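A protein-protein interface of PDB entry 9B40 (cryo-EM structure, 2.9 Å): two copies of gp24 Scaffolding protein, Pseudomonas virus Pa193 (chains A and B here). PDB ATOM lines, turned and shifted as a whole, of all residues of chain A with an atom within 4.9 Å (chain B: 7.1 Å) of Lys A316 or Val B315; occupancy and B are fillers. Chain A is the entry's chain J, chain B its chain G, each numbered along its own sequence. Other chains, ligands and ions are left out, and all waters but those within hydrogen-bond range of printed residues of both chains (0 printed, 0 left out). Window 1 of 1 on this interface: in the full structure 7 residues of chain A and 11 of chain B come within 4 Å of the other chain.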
ATOM      1  N   ILE A 312     -27.531 -10.986   6.817  1.00  0.00           N
ATOM      2  CA  ILE A 312     -27.333  -9.648   7.365  1.00  0.00           C
ATOM      3  C   ILE A 312     -26.287  -9.657   8.475  1.00  0.00           C
ATOM      4  O   ILE A 312     -25.550  -8.680   8.642  1.00  0.00           O
ATOM      5  CB  ILE A 312     -28.675  -9.050   7.825  1.00  0.00           C
ATOM      6  CG1 ILE A 312     -29.646  -9.026   6.650  1.00  0.00           C
ATOM      7  CG2 ILE A 312     -28.502  -7.637   8.353  1.00  0.00           C
ATOM      8  CD1 ILE A 312     -30.973  -8.407   6.973  1.00  0.00           C
ATOM      9  N   SER A 313     -26.180 -10.751   9.235  1.00  0.00           N
ATOM     10  CA  SER A 313     -25.097 -10.850  10.212  1.00  0.00           C
ATOM     11  C   SER A 313     -23.732 -10.839   9.530  1.00  0.00           C
ATOM     12  O   SER A 313     -22.805 -10.153   9.983  1.00  0.00           O
ATOM     13  CB  SER A 313     -25.266 -12.109  11.060  1.00  0.00           C
ATOM     14  OG  SER A 313     -24.641 -13.223  10.449  1.00  0.00           O
ATOM     15  N   GLN A 314     -23.593 -11.575   8.425  1.00  0.00           N
ATOM     16  CA  GLN A 314     -22.327 -11.566   7.695  1.00  0.00           C
ATOM     17  C   GLN A 314     -22.068 -10.212   7.039  1.00  0.00           C
ATOM     18  O   GLN A 314     -20.918  -9.761   6.973  1.00  0.00           O
ATOM     19  CB  GLN A 314     -22.299 -12.684   6.656  1.00  0.00           C
ATOM     20  CG  GLN A 314     -22.293 -14.084   7.244  1.00  0.00           C
ATOM     21  CD  GLN A 314     -23.238 -15.027   6.530  1.00  0.00           C
ATOM     22  OE1 GLN A 314     -23.485 -14.888   5.334  1.00  0.00           O
ATOM     23  NE2 GLN A 314     -23.779 -15.990   7.265  1.00  0.00           N
ATOM     24  N   VAL A 315     -23.120  -9.556   6.544  1.00  0.00           N
ATOM     25  CA  VAL A 315     -22.983  -8.208   5.996  1.00  0.00           C
ATOM     26  C   VAL A 315     -22.495  -7.244   7.071  1.00  0.00           C
ATOM     27  O   VAL A 315     -21.631  -6.395   6.821  1.00  0.00           O
ATOM     28  CB  VAL A 315     -24.319  -7.750   5.376  1.00  0.00           C
ATOM     29  CG1 VAL A 315     -24.360  -6.242   5.212  1.00  0.00           C
ATOM     30  CG2 VAL A 315     -24.531  -8.416   4.030  1.00  0.00           C
ATOM     31  N   LYS A 316     -23.027  -7.374   8.288  1.00  0.00           N
ATOM     32  CA  LYS A 316     -22.578  -6.533   9.391  1.00  0.00           C
ATOM     33  C   LYS A 316     -21.125  -6.822   9.743  1.00  0.00           C
ATOM     34  O   LYS A 316     -20.373  -5.909  10.100  1.00  0.00           O
ATOM     35  CB  LYS A 316     -23.470  -6.741  10.613  1.00  0.00           C
ATOM     36  CG  LYS A 316     -23.186  -5.757  11.726  1.00  0.00           C
ATOM     37  CD  LYS A 316     -23.935  -6.081  12.998  1.00  0.00           C
ATOM     38  CE  LYS A 316     -22.975  -6.569  14.062  1.00  0.00           C
ATOM     39  NZ  LYS A 316     -23.293  -5.996  15.397  1.00  0.00           N
ATOM     40  N   ALA A 317     -20.718  -8.092   9.667  1.00  0.00           N
ATOM     41  CA  ALA A 317     -19.316  -8.437   9.900  1.00  0.00           C
ATOM     42  C   ALA A 317     -18.404  -7.780   8.867  1.00  0.00           C
ATOM     43  O   ALA A 317     -17.347  -7.232   9.208  1.00  0.00           O
ATOM     44  CB  ALA A 317     -19.142  -9.956   9.879  1.00  0.00           C
ATOM     45  N   ILE A 318     -18.806  -7.823   7.592  1.00  0.00           N
ATOM     46  CA  ILE A 318     -18.028  -7.176   6.535  1.00  0.00           C
ATOM     47  C   ILE A 318     -17.971  -5.668   6.758  1.00  0.00           C
ATOM     48  O   ILE A 318     -16.933  -5.031   6.539  1.00  0.00           O
ATOM     49  CB  ILE A 318     -18.604  -7.529   5.150  1.00  0.00           C
ATOM     50  CG1 ILE A 318     -18.571  -9.043   4.925  1.00  0.00           C
ATOM     51  CG2 ILE A 318     -17.840  -6.812   4.045  1.00  0.00           C
ATOM     52  CD1 ILE A 318     -18.779  -9.463   3.484  1.00  0.00           C
ATOM     53  N   LEU A 319     -19.080  -5.075   7.210  1.00  0.00           N
ATOM     54  CA  LEU A 319     -19.096  -3.641   7.492  1.00  0.00           C
ATOM     55  C   LEU A 319     -18.187  -3.291   8.666  1.00  0.00           C
ATOM     56  O   LEU A 319     -17.530  -2.241   8.661  1.00  0.00           O
ATOM     57  CB  LEU A 319     -20.527  -3.179   7.760  1.00  0.00           C
ATOM     58  CG  LEU A 319     -21.168  -2.361   6.640  1.00  0.00           C
ATOM     59  CD1 LEU A 319     -22.666  -2.269   6.838  1.00  0.00           C
ATOM     60  CD2 LEU A 319     -20.553  -0.974   6.572  1.00  0.00           C
ATOM     61  N   ALA A 320     -18.144  -4.152   9.685  1.00  0.00           N
ATOM     62  CA  ALA A 320     -17.229  -3.940  10.801  1.00  0.00           C
ATOM     63  C   ALA A 320     -15.779  -4.011  10.341  1.00  0.00           C
ATOM     64  O   ALA A 320     -14.938  -3.220  10.786  1.00  0.00           O
ATOM     65  CB  ALA A 320     -17.494  -4.966  11.901  1.00  0.00           C
ATOM     66  N   ALA B 289     -16.850  -2.973  20.263  1.00  0.00           N
ATOM     67  CA  ALA B 289     -16.885  -4.331  19.739  1.00  0.00           C
ATOM     68  C   ALA B 289     -17.608  -5.298  20.664  1.00  0.00           C
ATOM     69  O   ALA B 289     -18.437  -6.085  20.199  1.00  0.00           O
ATOM     70  CB  ALA B 289     -15.464  -4.838  19.479  1.00  0.00           C
ATOM     71  N   GLU B 291     -19.850  -4.498  22.880  1.00  0.00           N
ATOM     72  CA  GLU B 291     -21.258  -4.121  22.789  1.00  0.00           C
ATOM     73  C   GLU B 291     -21.890  -4.665  21.514  1.00  0.00           C
ATOM     74  O   GLU B 291     -23.054  -5.083  21.519  1.00  0.00           O
ATOM     75  CB  GLU B 291     -21.404  -2.600  22.852  1.00  0.00           C
ATOM     76  CG  GLU B 291     -22.806  -2.109  23.211  1.00  0.00           C
ATOM     77  CD  GLU B 291     -23.268  -2.560  24.588  1.00  0.00           C
ATOM     78  OE1 GLU B 291     -22.412  -2.767  25.474  1.00  0.00           O
ATOM     79  OE2 GLU B 291     -24.493  -2.709  24.785  1.00  0.00           O
ATOM     80  N   SER B 292     -21.136  -4.667  20.411  1.00  0.00           N
ATOM     81  CA  SER B 292     -21.650  -5.215  19.160  1.00  0.00           C
ATOM     82  C   SER B 292     -21.911  -6.713  19.272  1.00  0.00           C
ATOM     83  O   SER B 292     -22.943  -7.201  18.801  1.00  0.00           O
ATOM     84  CB  SER B 292     -20.680  -4.919  18.019  1.00  0.00           C
ATOM     85  OG  SER B 292     -20.769  -3.562  17.618  1.00  0.00           O
ATOM     86  N   GLU B 293     -20.995  -7.462  19.894  1.00  0.00           N
ATOM     87  CA  GLU B 293     -21.240  -8.893  20.074  1.00  0.00           C
ATOM     88  C   GLU B 293     -22.357  -9.155  21.079  1.00  0.00           C
ATOM     89  O   GLU B 293     -23.092 -10.140  20.944  1.00  0.00           O
ATOM     90  CB  GLU B 293     -19.961  -9.641  20.485  1.00  0.00           C
ATOM     91  CG  GLU B 293     -18.578  -9.222  19.904  1.00  0.00           C
ATOM     92  CD  GLU B 293     -18.557  -8.673  18.467  1.00  0.00           C
ATOM     93  OE1 GLU B 293     -19.422  -9.018  17.632  1.00  0.00           O
ATOM     94  OE2 GLU B 293     -17.639  -7.882  18.166  1.00  0.00           O
ATOM     95  N   GLN B 295     -25.011  -7.218  21.419  1.00  0.00           N
ATOM     96  CA  GLN B 295     -26.207  -6.989  20.616  1.00  0.00           C
ATOM     97  C   GLN B 295     -26.445  -8.132  19.635  1.00  0.00           C
ATOM     98  O   GLN B 295     -27.593  -8.496  19.372  1.00  0.00           O
ATOM     99  CB  GLN B 295     -26.090  -5.658  19.875  1.00  0.00           C
ATOM    100  CG  GLN B 295     -26.365  -4.444  20.742  1.00  0.00           C
ATOM    101  CD  GLN B 295     -25.894  -3.155  20.103  1.00  0.00           C
ATOM    102  OE1 GLN B 295     -24.748  -3.046  19.668  1.00  0.00           O
ATOM    103  NE2 GLN B 295     -26.777  -2.166  20.047  1.00  0.00           N
ATOM    104  N   GLU B 296     -25.372  -8.702  19.078  1.00  0.00           N
ATOM    105  CA  GLU B 296     -25.508  -9.858  18.193  1.00  0.00           C
ATOM    106  C   GLU B 296     -26.100 -11.056  18.921  1.00  0.00           C
ATOM    107  O   GLU B 296     -27.008 -11.723  18.407  1.00  0.00           O
ATOM    108  CB  GLU B 296     -24.155 -10.229  17.590  1.00  0.00           C
ATOM    109  CG  GLU B 296     -24.252 -11.214  16.435  1.00  0.00           C
ATOM    110  CD  GLU B 296     -24.073 -10.565  15.086  1.00  0.00           C
ATOM    111  OE1 GLU B 296     -23.824 -11.292  14.103  1.00  0.00           O
ATOM    112  OE2 GLU B 296     -24.194  -9.330  15.006  1.00  0.00           O
ATOM    113  N   ALA B 309     -34.691  -6.978  12.515  1.00  0.00           N
ATOM    114  CA  ALA B 309     -34.810  -5.555  12.813  1.00  0.00           C
ATOM    115  C   ALA B 309     -33.582  -5.039  13.552  1.00  0.00           C
ATOM    116  O   ALA B 309     -33.008  -4.009  13.178  1.00  0.00           O
ATOM    117  CB  ALA B 309     -36.074  -5.302  13.632  1.00  0.00           C
ATOM    118  N   GLU B 310     -33.153  -5.751  14.598  1.00  0.00           N
ATOM    119  CA  GLU B 310     -31.978  -5.309  15.346  1.00  0.00           C
ATOM    120  C   GLU B 310     -30.702  -5.424  14.525  1.00  0.00           C
ATOM    121  O   GLU B 310     -29.811  -4.581  14.658  1.00  0.00           O
ATOM    122  CB  GLU B 310     -31.844  -6.077  16.658  1.00  0.00           C
ATOM    123  CG  GLU B 310     -32.838  -5.657  17.722  1.00  0.00           C
ATOM    124  CD  GLU B 310     -32.687  -4.203  18.132  1.00  0.00           C
ATOM    125  OE1 GLU B 310     -31.543  -3.702  18.146  1.00  0.00           O
ATOM    126  OE2 GLU B 310     -33.711  -3.565  18.450  1.00  0.00           O
ATOM    127  N   LEU B 311     -30.580  -6.452  13.681  1.00  0.00           N
ATOM    128  CA  LEU B 311     -29.393  -6.546  12.835  1.00  0.00           C
ATOM    129  C   LEU B 311     -29.320  -5.388  11.851  1.00  0.00           C
ATOM    130  O   LEU B 311     -28.246  -4.809  11.649  1.00  0.00           O
ATOM    131  CB  LEU B 311     -29.349  -7.879  12.091  1.00  0.00           C
ATOM    132  CG  LEU B 311     -29.079  -9.140  12.909  1.00  0.00           C
ATOM    133  CD1 LEU B 311     -29.395 -10.376  12.086  1.00  0.00           C
ATOM    134  CD2 LEU B 311     -27.639  -9.158  13.387  1.00  0.00           C
ATOM    135  N   ILE B 312     -30.447  -5.021  11.236  1.00  0.00           N
ATOM    136  CA  ILE B 312     -30.411  -3.883  10.325  1.00  0.00           C
ATOM    137  C   ILE B 312     -30.187  -2.579  11.089  1.00  0.00           C
ATOM    138  O   ILE B 312     -29.536  -1.660  10.578  1.00  0.00           O
ATOM    139  CB  ILE B 312     -31.678  -3.865   9.449  1.00  0.00           C
ATOM    140  CG1 ILE B 312     -31.666  -5.085   8.529  1.00  0.00           C
ATOM    141  CG2 ILE B 312     -31.754  -2.613   8.595  1.00  0.00           C
ATOM    142  CD1 ILE B 312     -32.881  -5.216   7.664  1.00  0.00           C
ATOM    143  N   SER B 313     -30.675  -2.481  12.331  1.00  0.00           N
ATOM    144  CA  SER B 313     -30.387  -1.299  13.143  1.00  0.00           C
ATOM    145  C   SER B 313     -28.897  -1.183  13.458  1.00  0.00           C
ATOM    146  O   SER B 313     -28.326  -0.086  13.403  1.00  0.00           O
ATOM    147  CB  SER B 313     -31.204  -1.331  14.432  1.00  0.00           C
ATOM    148  OG  SER B 313     -30.428  -1.805  15.517  1.00  0.00           O
ATOM    149  N   GLN B 314     -28.247  -2.301  13.795  1.00  0.00           N
ATOM    150  CA  GLN B 314     -26.806  -2.272  14.045  1.00  0.00           C
ATOM    151  C   GLN B 314     -26.025  -1.973  12.771  1.00  0.00           C
ATOM    152  O   GLN B 314     -24.999  -1.282  12.812  1.00  0.00           O
ATOM    153  CB  GLN B 314     -26.343  -3.588  14.667  1.00  0.00           C
ATOM    154  CG  GLN B 314     -27.029  -3.932  15.975  1.00  0.00           C
ATOM    155  CD  GLN B 314     -26.988  -5.414  16.282  1.00  0.00           C
ATOM    156  OE1 GLN B 314     -26.109  -6.133  15.813  1.00  0.00           O
ATOM    157  NE2 GLN B 314     -27.952  -5.881  17.066  1.00  0.00           N
ATOM    158  N   VAL B 315     -26.492  -2.491  11.631  1.00  0.00           N
ATOM    159  CA  VAL B 315     -25.884  -2.149  10.348  1.00  0.00           C
ATOM    160  C   VAL B 315     -25.994  -0.650  10.092  1.00  0.00           C
ATOM    161  O   VAL B 315     -25.041  -0.012   9.626  1.00  0.00           O
ATOM    162  CB  VAL B 315     -26.529  -2.976   9.218  1.00  0.00           C
ATOM    163  CG1 VAL B 315     -26.213  -2.386   7.858  1.00  0.00           C
ATOM    164  CG2 VAL B 315     -26.048  -4.414   9.280  1.00  0.00           C
ATOM    165  N   LYS B 316     -27.150  -0.064  10.414  1.00  0.00           N
ATOM    166  CA  LYS B 316     -27.327   1.374  10.251  1.00  0.00           C
ATOM    167  C   LYS B 316     -26.393   2.150  11.171  1.00  0.00           C
ATOM    168  O   LYS B 316     -25.840   3.182  10.779  1.00  0.00           O
ATOM    169  CB  LYS B 316     -28.779   1.766  10.520  1.00  0.00           C
ATOM    170  CG  LYS B 316     -28.983   3.265  10.635  1.00  0.00           C
ATOM    171  CD  LYS B 316     -30.435   3.659  10.760  1.00  0.00           C
ATOM    172  CE  LYS B 316     -30.554   5.172  10.780  1.00  0.00           C
ATOM    173  NZ  LYS B 316     -30.988   5.714  12.089  1.00  0.00           N
ATOM    174  N   ALA B 317     -26.216   1.671  12.405  1.00  0.00           N
ATOM    175  CA  ALA B 317     -25.303   2.333  13.334  1.00  0.00           C
ATOM    176  C   ALA B 317     -23.868   2.302  12.822  1.00  0.00           C
ATOM    177  O   ALA B 317     -23.149   3.308  12.897  1.00  0.00           O
ATOM    178  CB  ALA B 317     -25.394   1.682  14.713  1.00  0.00           C
ATOM    179  N   ILE B 318     -23.434   1.156  12.289  1.00  0.00           N
ATOM    180  CA  ILE B 318     -22.090   1.065  11.719  1.00  0.00           C
ATOM    181  C   ILE B 318     -21.954   1.977  10.503  1.00  0.00           C
ATOM    182  O   ILE B 318     -20.918   2.622  10.312  1.00  0.00           O
ATOM    183  CB  ILE B 318     -21.738  -0.396  11.381  1.00  0.00           C
ATOM    184  CG1 ILE B 318     -21.744  -1.245  12.648  1.00  0.00           C
ATOM    185  CG2 ILE B 318     -20.381  -0.491  10.702  1.00  0.00           C
ATOM    186  CD1 ILE B 318     -21.436  -2.690  12.397  1.00  0.00           C
ATOM    187  N   LEU B 319     -22.993   2.049   9.667  1.00  0.00           N
ATOM    188  CA  LEU B 319     -22.948   2.939   8.508  1.00  0.00           C
ATOM    189  C   LEU B 319     -22.879   4.404   8.929  1.00  0.00           C
ATOM    190  O   LEU B 319     -22.166   5.204   8.309  1.00  0.00           O
ATOM    191  CB  LEU B 319     -24.161   2.694   7.611  1.00  0.00           C
ATOM    192  CG  LEU B 319     -23.978   1.648   6.510  1.00  0.00           C
ATOM    193  CD1 LEU B 319     -25.324   1.159   6.006  1.00  0.00           C
ATOM    194  CD2 LEU B 319     -23.149   2.210   5.367  1.00  0.00           C
ATOM    195  N   ALA B 320     -23.616   4.772   9.977  1.00  0.00           N
ATOM    196  CA  ALA B 320     -23.558   6.135  10.494  1.00  0.00           C
ATOM    197  C   ALA B 320     -22.178   6.455  11.050  1.00  0.00           C
ATOM    198  O   ALA B 320     -21.670   7.566  10.867  1.00  0.00           O
ATOM    199  CB  ALA B 320     -24.629   6.337  11.564  1.00  0.00           C
ATOM    200  N   ARG B 321     -21.556   5.494  11.739  1.00  0.00           N
ATOM    201  CA  ARG B 321     -20.194   5.712  12.224  1.00  0.00           C
ATOM    202  C   ARG B 321     -19.202   5.817  11.068  1.00  0.00           C
ATOM    203  O   ARG B 321     -18.242   6.594  11.138  1.00  0.00           O
ATOM    204  CB  ARG B 321     -19.797   4.600  13.195  1.00  0.00           C
ATOM    205  CG  ARG B 321     -20.436   4.760  14.567  1.00  0.00           C
ATOM    206  CD  ARG B 321     -20.629   3.435  15.288  1.00  0.00           C
ATOM    207  NE  ARG B 321     -19.396   2.663  15.384  1.00  0.00           N
ATOM    208  CZ  ARG B 321     -19.336   1.340  15.343  1.00  0.00           C
ATOM    209  NH1 ARG B 321     -20.423   0.604  15.185  1.00  0.00           N
ATOM    210  NH2 ARG B 321     -18.157   0.739  15.472  1.00  0.00           N
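Hydrophobic or aromatic side chains of chain B within 4 Å of the printed part of chain A: Leu B311, Ile B312, Val B315 and Ile B318.
Of the 9 printed residues of chain A, 4 touch a printed residue of chain B.
Hydrophobic or aromatic side chains of chain A that line the printed part of chain B: Ile A312 and Leu A319.
Among the printed residues, 10 pairs touch across the chains.
Among the printed residues, Asp or Glu carboxylates within 4 Å of a Lys or Arg side-chain nitrogen of the other chain: Lys A316 with Glu B296 (3.5 Å).
Ile A312 touches its own counterpart, Ile B312.
Lys A316 touches Val B315, but with the chains exchanged Val A315 does not touch Lys B316 (8.5 Å).
Lys A316 touches Ile B318, but with the chains exchanged Ile A318 does not touch Lys B316 (11.4 Å).
Leu A319 touches Val B315, but with the chains exchanged Val A315 does not touch Leu B319 (7.5 Å).
The side-chain carboxylate (OE2) of Glu B296 lies within salt-bridge range of the side-chain amino group (NZ) of Lys A316 (3.5 Å).
The side-chain amide oxygen of Gln B314 lies within hydrogen-bond range of the side-chain amino group of Lys A316, at 2.8 Å.
Ile A318 touches none of the printed residues of chain B.
Of the printed residues of chain B, Leu A319 touches Val B315 and Ile B318.
Of the printed residues of chain A, Glu B296 touches Ser A313 and Lys A316.
Ala B309 touches none of the printed residues of chain A.
Of the printed residues of chain A, Ile B312 touches Ile A312 (3.7 Å).
Of the printed residues of chain A, Gln B314 touches Lys A316.
Val B315 touches just these residues of chain A: Lys A316 and Leu A319.
Printed residues of chain A within 4 Å of Ile B318: Lys A316 (3.6 Å) and Leu A319 (3.9 Å).
The backbone carbonyl oxygen (O) of Glu B310 sits close to the side-chain amide nitrogen (NE2) of Gln B314 (3.3 Å).
Among the printed residues, pairs that only touch across the chains: Ser A313 with Glu B296 (3.5 Å), Lys A316 with Ile B318 (3.6 Å), Lys A316 with Ser B292 (3.6 Å), Leu A319 with Val B315 (3.7 Å), Lys A316 with Val B315 (3.7 Å), Ile A312 with Ile B312 (3.7 Å), Ile A312 with Leu B311 (3.8 Å) and Leu A319 with Ile B318 (3.9 Å).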
